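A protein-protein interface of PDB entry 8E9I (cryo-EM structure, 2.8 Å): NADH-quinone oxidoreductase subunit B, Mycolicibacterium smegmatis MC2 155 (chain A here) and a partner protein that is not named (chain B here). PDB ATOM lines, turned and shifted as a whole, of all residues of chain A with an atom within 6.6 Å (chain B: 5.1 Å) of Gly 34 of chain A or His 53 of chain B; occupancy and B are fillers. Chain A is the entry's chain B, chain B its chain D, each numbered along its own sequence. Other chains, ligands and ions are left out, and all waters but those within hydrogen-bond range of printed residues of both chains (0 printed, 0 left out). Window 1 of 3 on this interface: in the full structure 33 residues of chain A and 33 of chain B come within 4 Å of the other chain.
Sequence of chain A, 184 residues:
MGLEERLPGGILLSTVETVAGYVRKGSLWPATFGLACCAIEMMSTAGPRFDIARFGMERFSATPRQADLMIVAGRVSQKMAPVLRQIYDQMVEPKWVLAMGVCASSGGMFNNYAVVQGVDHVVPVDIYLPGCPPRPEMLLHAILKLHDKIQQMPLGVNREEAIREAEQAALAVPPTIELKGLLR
Gly 34 of chain A touches two residues of chain B.
Printed residues of chain B within 4 Å of Leu 35 of chain A: Val 55.
His 53 of chain B touches just one residue of chain A: Gly 34.
Printed residues of chain A within 4 Å of Gly 54 of chain B: Gly 34 (3.3 Å).
Of the printed residues of chain A, Val 55 of chain B touches Leu 35 (3.8 Å).
The nearest residue of chain B that does not touch Gly 34 of chain A is Val 55 of chain B (4.7 Å).
The nearest printed residue of chain B that does not touch Leu 35 of chain A is His 53 of chain B (4.3 Å).
Among the printed residues, merely in contact across the chains: Gly 34 of chain A with His 53 of chain B (3.7 Å), Gly 34 of chain A with Gly 54 of chain B (3.3 Å) and Leu 35 of chain A with Val 55 of chain B (3.8 Å).
Hydrophobic or aromatic side chains of chain B within 4 Å of the printed part of chain A: Val 55.
Of the 14 printed residues of chain A, 2 touch a printed residue of chain B.
Among the printed residues, 3 pairs touch across the chains.
N of Leu 35 of chain A lies within hydrogen-bond range of O of Ala 73 of chain A (3.2 Å).
The backbone carbonyl oxygen of Pro 47 of chain B sits close to the backbone NH of Gly 54 of chain B (3.3 Å).
The backbone carbonyl oxygen of Pro 435 of chain B lies close to a ring nitrogen (NE2) of His 53 of chain B, 3.4 Å away.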
ATOM      1  N   ALA A  31      -4.575  -5.285 -15.970  1.00  0.00           N
ATOM      2  CA  ALA A  31      -3.419  -5.455 -15.101  1.00  0.00           C
ATOM      3  C   ALA A  31      -2.885  -4.092 -14.688  1.00  0.00           C
ATOM      4  O   ALA A  31      -2.894  -3.141 -15.473  1.00  0.00           O
ATOM      5  CB  ALA A  31      -2.325  -6.251 -15.808  1.00  0.00           C
ATOM      6  N   THR A  32      -2.431  -3.991 -13.442  1.00  0.00           N
ATOM      7  CA  THR A  32      -1.851  -2.748 -12.938  1.00  0.00           C
ATOM      8  C   THR A  32      -0.471  -2.588 -13.562  1.00  0.00           C
ATOM      9  O   THR A  32       0.567  -2.802 -12.931  1.00  0.00           O
ATOM     10  CB  THR A  32      -1.772  -2.760 -11.420  1.00  0.00           C
ATOM     11  OG1 THR A  32      -3.040  -3.143 -10.880  1.00  0.00           O
ATOM     12  CG2 THR A  32      -1.387  -1.389 -10.901  1.00  0.00           C
ATOM     13  N   PHE A  33      -0.464  -2.203 -14.837  1.00  0.00           N
ATOM     14  CA  PHE A  33       0.769  -2.209 -15.607  1.00  0.00           C
ATOM     15  C   PHE A  33       0.937  -0.960 -16.454  1.00  0.00           C
ATOM     16  O   PHE A  33       1.164  -1.052 -17.663  1.00  0.00           O
ATOM     17  CB  PHE A  33       0.823  -3.446 -16.497  1.00  0.00           C
ATOM     18  CG  PHE A  33       2.132  -3.625 -17.193  1.00  0.00           C
ATOM     19  CD1 PHE A  33       3.322  -3.471 -16.511  1.00  0.00           C
ATOM     20  CD2 PHE A  33       2.174  -3.956 -18.528  1.00  0.00           C
ATOM     21  CE1 PHE A  33       4.522  -3.636 -17.148  1.00  0.00           C
ATOM     22  CE2 PHE A  33       3.371  -4.122 -19.166  1.00  0.00           C
ATOM     23  CZ  PHE A  33       4.549  -3.965 -18.474  1.00  0.00           C
ATOM     24  N   GLY A  34       0.806   0.213 -15.842  1.00  0.00           N
ATOM     25  CA  GLY A  34       1.132   1.443 -16.538  1.00  0.00           C
ATOM     26  C   GLY A  34       2.627   1.540 -16.796  1.00  0.00           C
ATOM     27  O   GLY A  34       3.440   0.962 -16.080  1.00  0.00           O
ATOM     28  N   LEU A  35       2.982   2.274 -17.846  1.00  0.00           N
ATOM     29  CA  LEU A  35       4.375   2.488 -18.215  1.00  0.00           C
ATOM     30  C   LEU A  35       4.769   3.958 -18.218  1.00  0.00           C
ATOM     31  O   LEU A  35       5.808   4.321 -17.668  1.00  0.00           O
ATOM     32  CB  LEU A  35       4.650   1.887 -19.595  1.00  0.00           C
ATOM     33  CG  LEU A  35       5.306   0.511 -19.616  1.00  0.00           C
ATOM     34  CD1 LEU A  35       4.480  -0.478 -18.843  1.00  0.00           C
ATOM     35  CD2 LEU A  35       5.482   0.041 -21.037  1.00  0.00           C
ATOM     36  N   ALA A  36       3.960   4.811 -18.829  1.00  0.00           N
ATOM     37  CA  ALA A  36       4.375   6.176 -19.105  1.00  0.00           C
ATOM     38  C   ALA A  36       3.169   7.100 -19.140  1.00  0.00           C
ATOM     39  O   ALA A  36       2.132   6.797 -18.546  1.00  0.00           O
ATOM     40  CB  ALA A  36       5.154   6.231 -20.417  1.00  0.00           C
ATOM     41  N   CYS A  38       0.785   7.493 -20.916  1.00  0.00           N
ATOM     42  CA  CYS A  38      -0.476   6.800 -21.099  1.00  0.00           C
ATOM     43  C   CYS A  38      -0.931   6.135 -19.811  1.00  0.00           C
ATOM     44  O   CYS A  38      -2.128   5.940 -19.612  1.00  0.00           O
ATOM     45  CB  CYS A  38      -0.339   5.781 -22.226  1.00  0.00           C
ATOM     46  SG  CYS A  38      -0.083   6.513 -23.853  1.00  0.00           S
ATOM     47  N   ALA A  39      -0.003   5.794 -18.919  1.00  0.00           N
ATOM     48  CA  ALA A  39      -0.408   5.276 -17.617  1.00  0.00           C
ATOM     49  C   ALA A  39      -1.137   6.333 -16.809  1.00  0.00           C
ATOM     50  O   ALA A  39      -2.137   6.034 -16.148  1.00  0.00           O
ATOM     51  CB  ALA A  39       0.806   4.777 -16.843  1.00  0.00           C
ATOM     52  N   ILE A  40      -0.652   7.572 -16.849  1.00  0.00           N
ATOM     53  CA  ILE A  40      -1.363   8.652 -16.183  1.00  0.00           C
ATOM     54  C   ILE A  40      -2.744   8.821 -16.789  1.00  0.00           C
ATOM     55  O   ILE A  40      -3.730   8.995 -16.067  1.00  0.00           O
ATOM     56  CB  ILE A  40      -0.552   9.957 -16.255  1.00  0.00           C
ATOM     57  CG1 ILE A  40       0.862   9.746 -15.710  1.00  0.00           C
ATOM     58  CG2 ILE A  40      -1.280  11.072 -15.551  1.00  0.00           C
ATOM     59  CD1 ILE A  40       0.923   9.201 -14.311  1.00  0.00           C
ATOM     60  N   MET A  42      -4.481   6.545 -18.175  1.00  0.00           N
ATOM     61  CA  MET A  42      -5.265   5.390 -17.758  1.00  0.00           C
ATOM     62  C   MET A  42      -5.805   5.591 -16.347  1.00  0.00           C
ATOM     63  O   MET A  42      -6.973   5.298 -16.061  1.00  0.00           O
ATOM     64  CB  MET A  42      -4.401   4.134 -17.855  1.00  0.00           C
ATOM     65  CG  MET A  42      -5.105   2.846 -17.504  1.00  0.00           C
ATOM     66  SD  MET A  42      -4.012   1.429 -17.675  1.00  0.00           S
ATOM     67  CE  MET A  42      -2.923   1.663 -16.280  1.00  0.00           C
ATOM     68  N   ILE A  71      -3.343  -3.306 -20.607  1.00  0.00           N
ATOM     69  CA  ILE A  71      -3.214  -1.997 -21.237  1.00  0.00           C
ATOM     70  C   ILE A  71      -1.744  -1.618 -21.168  1.00  0.00           C
ATOM     71  O   ILE A  71      -1.258  -1.183 -20.123  1.00  0.00           O
ATOM     72  CB  ILE A  71      -4.085  -0.938 -20.555  1.00  0.00           C
ATOM     73  CG1 ILE A  71      -5.487  -1.472 -20.292  1.00  0.00           C
ATOM     74  CG2 ILE A  71      -4.169   0.294 -21.421  1.00  0.00           C
ATOM     75  CD1 ILE A  71      -6.377  -0.520 -19.552  1.00  0.00           C
ATOM     76  N   VAL A  72      -1.026  -1.787 -22.276  1.00  0.00           N
ATOM     77  CA  VAL A  72       0.393  -1.464 -22.262  1.00  0.00           C
ATOM     78  C   VAL A  72       0.601  -0.021 -21.837  1.00  0.00           C
ATOM     79  O   VAL A  72       1.397   0.265 -20.936  1.00  0.00           O
ATOM     80  CB  VAL A  72       1.017  -1.754 -23.632  1.00  0.00           C
ATOM     81  CG1 VAL A  72       2.392  -1.138 -23.719  1.00  0.00           C
ATOM     82  CG2 VAL A  72       1.099  -3.246 -23.841  1.00  0.00           C
ATOM     83  N   ALA A  73      -0.117   0.907 -22.461  1.00  0.00           N
ATOM     84  CA  ALA A  73      -0.207   2.277 -21.970  1.00  0.00           C
ATOM     85  C   ALA A  73       1.168   2.839 -21.627  1.00  0.00           C
ATOM     86  O   ALA A  73       1.467   3.173 -20.481  1.00  0.00           O
ATOM     87  CB  ALA A  73      -1.133   2.347 -20.758  1.00  0.00           C
ATOM     88  N   GLY A  74       2.017   2.943 -22.641  1.00  0.00           N
ATOM     89  CA  GLY A  74       3.314   3.557 -22.445  1.00  0.00           C
ATOM     90  C   GLY A  74       4.291   3.064 -23.486  1.00  0.00           C
ATOM     91  O   GLY A  74       3.927   2.306 -24.382  1.00  0.00           O
ATOM     92  N   PRO B  47       9.601  -3.859 -11.809  1.00  0.00           N
ATOM     93  CA  PRO B  47       8.897  -2.870 -12.625  1.00  0.00           C
ATOM     94  C   PRO B  47       7.396  -2.962 -12.433  1.00  0.00           C
ATOM     95  O   PRO B  47       6.755  -1.983 -12.047  1.00  0.00           O
ATOM     96  CB  PRO B  47       9.324  -3.228 -14.053  1.00  0.00           C
ATOM     97  CG  PRO B  47      10.602  -3.982 -13.881  1.00  0.00           C
ATOM     98  CD  PRO B  47      10.412  -4.764 -12.636  1.00  0.00           C
ATOM     99  N   HIS B  49       4.736  -3.397 -10.479  1.00  0.00           N
ATOM    100  CA  HIS B  49       4.329  -3.418  -9.086  1.00  0.00           C
ATOM    101  C   HIS B  49       3.507  -2.166  -8.841  1.00  0.00           C
ATOM    102  O   HIS B  49       3.881  -1.087  -9.312  1.00  0.00           O
ATOM    103  CB  HIS B  49       5.550  -3.475  -8.161  1.00  0.00           C
ATOM    104  CG  HIS B  49       5.225  -3.652  -6.713  1.00  0.00           C
ATOM    105  ND1 HIS B  49       4.516  -2.721  -5.986  1.00  0.00           N
ATOM    106  CD2 HIS B  49       5.537  -4.644  -5.847  1.00  0.00           C
ATOM    107  CE1 HIS B  49       4.392  -3.139  -4.740  1.00  0.00           C
ATOM    108  NE2 HIS B  49       5.003  -4.303  -4.629  1.00  0.00           N
ATOM    109  N   PRO B  50       2.383  -2.271  -8.137  1.00  0.00           N
ATOM    110  CA  PRO B  50       1.479  -1.116  -8.060  1.00  0.00           C
ATOM    111  C   PRO B  50       2.137   0.140  -7.527  1.00  0.00           C
ATOM    112  O   PRO B  50       1.761   1.243  -7.938  1.00  0.00           O
ATOM    113  CB  PRO B  50       0.367  -1.614  -7.129  1.00  0.00           C
ATOM    114  CG  PRO B  50       0.368  -3.080  -7.314  1.00  0.00           C
ATOM    115  CD  PRO B  50       1.798  -3.461  -7.495  1.00  0.00           C
ATOM    116  N   SER B  51       3.106   0.013  -6.625  1.00  0.00           N
ATOM    117  CA  SER B  51       3.719   1.183  -6.015  1.00  0.00           C
ATOM    118  C   SER B  51       4.898   1.736  -6.804  1.00  0.00           C
ATOM    119  O   SER B  51       5.347   2.846  -6.509  1.00  0.00           O
ATOM    120  CB  SER B  51       4.188   0.844  -4.604  1.00  0.00           C
ATOM    121  OG  SER B  51       5.357   0.049  -4.649  1.00  0.00           O
ATOM    122  N   THR B  52       5.414   1.008  -7.792  1.00  0.00           N
ATOM    123  CA  THR B  52       6.645   1.400  -8.465  1.00  0.00           C
ATOM    124  C   THR B  52       6.412   2.068  -9.811  1.00  0.00           C
ATOM    125  O   THR B  52       7.363   2.228 -10.579  1.00  0.00           O
ATOM    126  CB  THR B  52       7.555   0.192  -8.653  1.00  0.00           C
ATOM    127  OG1 THR B  52       6.848  -0.827  -9.365  1.00  0.00           O
ATOM    128  CG2 THR B  52       8.018  -0.338  -7.305  1.00  0.00           C
ATOM    129  N   HIS B  53       5.180   2.452 -10.124  1.00  0.00           N
ATOM    130  CA  HIS B  53       4.907   3.182 -11.356  1.00  0.00           C
ATOM    131  C   HIS B  53       5.259   2.354 -12.587  1.00  0.00           C
ATOM    132  O   HIS B  53       5.435   2.890 -13.682  1.00  0.00           O
ATOM    133  CB  HIS B  53       5.662   4.510 -11.381  1.00  0.00           C
ATOM    134  CG  HIS B  53       5.617   5.252 -10.084  1.00  0.00           C
ATOM    135  ND1 HIS B  53       4.437   5.669  -9.508  1.00  0.00           N
ATOM    136  CD2 HIS B  53       6.604   5.641  -9.245  1.00  0.00           C
ATOM    137  CE1 HIS B  53       4.700   6.290  -8.374  1.00  0.00           C
ATOM    138  NE2 HIS B  53       6.007   6.286  -8.190  1.00  0.00           N
ATOM    139  N   GLY B  54       5.379   1.043 -12.418  1.00  0.00           N
ATOM    140  CA  GLY B  54       5.470   0.151 -13.554  1.00  0.00           C
ATOM    141  C   GLY B  54       6.846  -0.035 -14.159  1.00  0.00           C
ATOM    142  O   GLY B  54       7.094  -1.061 -14.796  1.00  0.00           O
ATOM    143  N   VAL B  55       7.745   0.932 -13.991  1.00  0.00           N
ATOM    144  CA  VAL B  55       9.028   0.882 -14.686  1.00  0.00           C
ATOM    145  C   VAL B  55      10.195   1.199 -13.758  1.00  0.00           C
ATOM    146  O   VAL B  55      11.283   1.562 -14.217  1.00  0.00           O
ATOM    147  CB  VAL B  55       9.024   1.828 -15.899  1.00  0.00           C
ATOM    148  CG1 VAL B  55       8.048   1.326 -16.944  1.00  0.00           C
ATOM    149  CG2 VAL B  55       8.676   3.235 -15.470  1.00  0.00           C
ATOM    150  N   LEU B  56       9.980   1.085 -12.456  1.00  0.00           N
ATOM    151  CA  LEU B  56      11.030   1.294 -11.470  1.00  0.00           C
ATOM    152  C   LEU B  56      11.259  -0.005 -10.713  1.00  0.00           C
ATOM    153  O   LEU B  56      10.298  -0.629 -10.259  1.00  0.00           O
ATOM    154  CB  LEU B  56      10.639   2.417 -10.512  1.00  0.00           C
ATOM    155  CG  LEU B  56      11.534   2.625  -9.300  1.00  0.00           C
ATOM    156  CD1 LEU B  56      12.971   2.874  -9.699  1.00  0.00           C
ATOM    157  CD2 LEU B  56      11.007   3.778  -8.481  1.00  0.00           C
ATOM    158  N   THR B 152      -1.273   8.898  -6.166  1.00  0.00           N
ATOM    159  CA  THR B 152      -0.562   7.639  -6.324  1.00  0.00           C
ATOM    160  C   THR B 152       0.003   7.168  -4.990  1.00  0.00           C
ATOM    161  O   THR B 152      -0.039   5.974  -4.677  1.00  0.00           O
ATOM    162  CB  THR B 152       0.537   7.782  -7.381  1.00  0.00           C
ATOM    163  OG1 THR B 152       1.050   6.490  -7.718  1.00  0.00           O
ATOM    164  CG2 THR B 152       1.675   8.660  -6.894  1.00  0.00           C
ATOM    165  N   PRO B 435       8.723   9.838  -7.517  1.00  0.00           N
ATOM    166  CA  PRO B 435       9.505   9.678  -8.745  1.00  0.00           C
ATOM    167  C   PRO B 435       8.610   9.458  -9.950  1.00  0.00           C
ATOM    168  O   PRO B 435       7.809   8.522  -9.988  1.00  0.00           O
ATOM    169  CB  PRO B 435      10.358   8.442  -8.455  1.00  0.00           C
ATOM    170  CG  PRO B 435       9.514   7.638  -7.540  1.00  0.00           C
ATOM    171  CD  PRO B 435       8.754   8.621  -6.690  1.00  0.00           C
ATOM    172  N   MET B 437       8.965   8.296 -13.549  1.00  0.00           N
ATOM    173  CA  MET B 437      10.033   7.543 -14.186  1.00  0.00           C
ATOM    174  C   MET B 437      10.339   8.021 -15.594  1.00  0.00           C
ATOM    175  O   MET B 437      11.440   7.764 -16.093  1.00  0.00           O
ATOM    176  CB  MET B 437       9.678   6.057 -14.210  1.00  0.00           C
ATOM    177  CG  MET B 437       9.590   5.411 -12.833  1.00  0.00           C
ATOM    178  SD  MET B 437      10.866   5.968 -11.689  1.00  0.00           S
ATOM    179  CE  MET B 437      12.298   5.157 -12.382  1.00  0.00           C
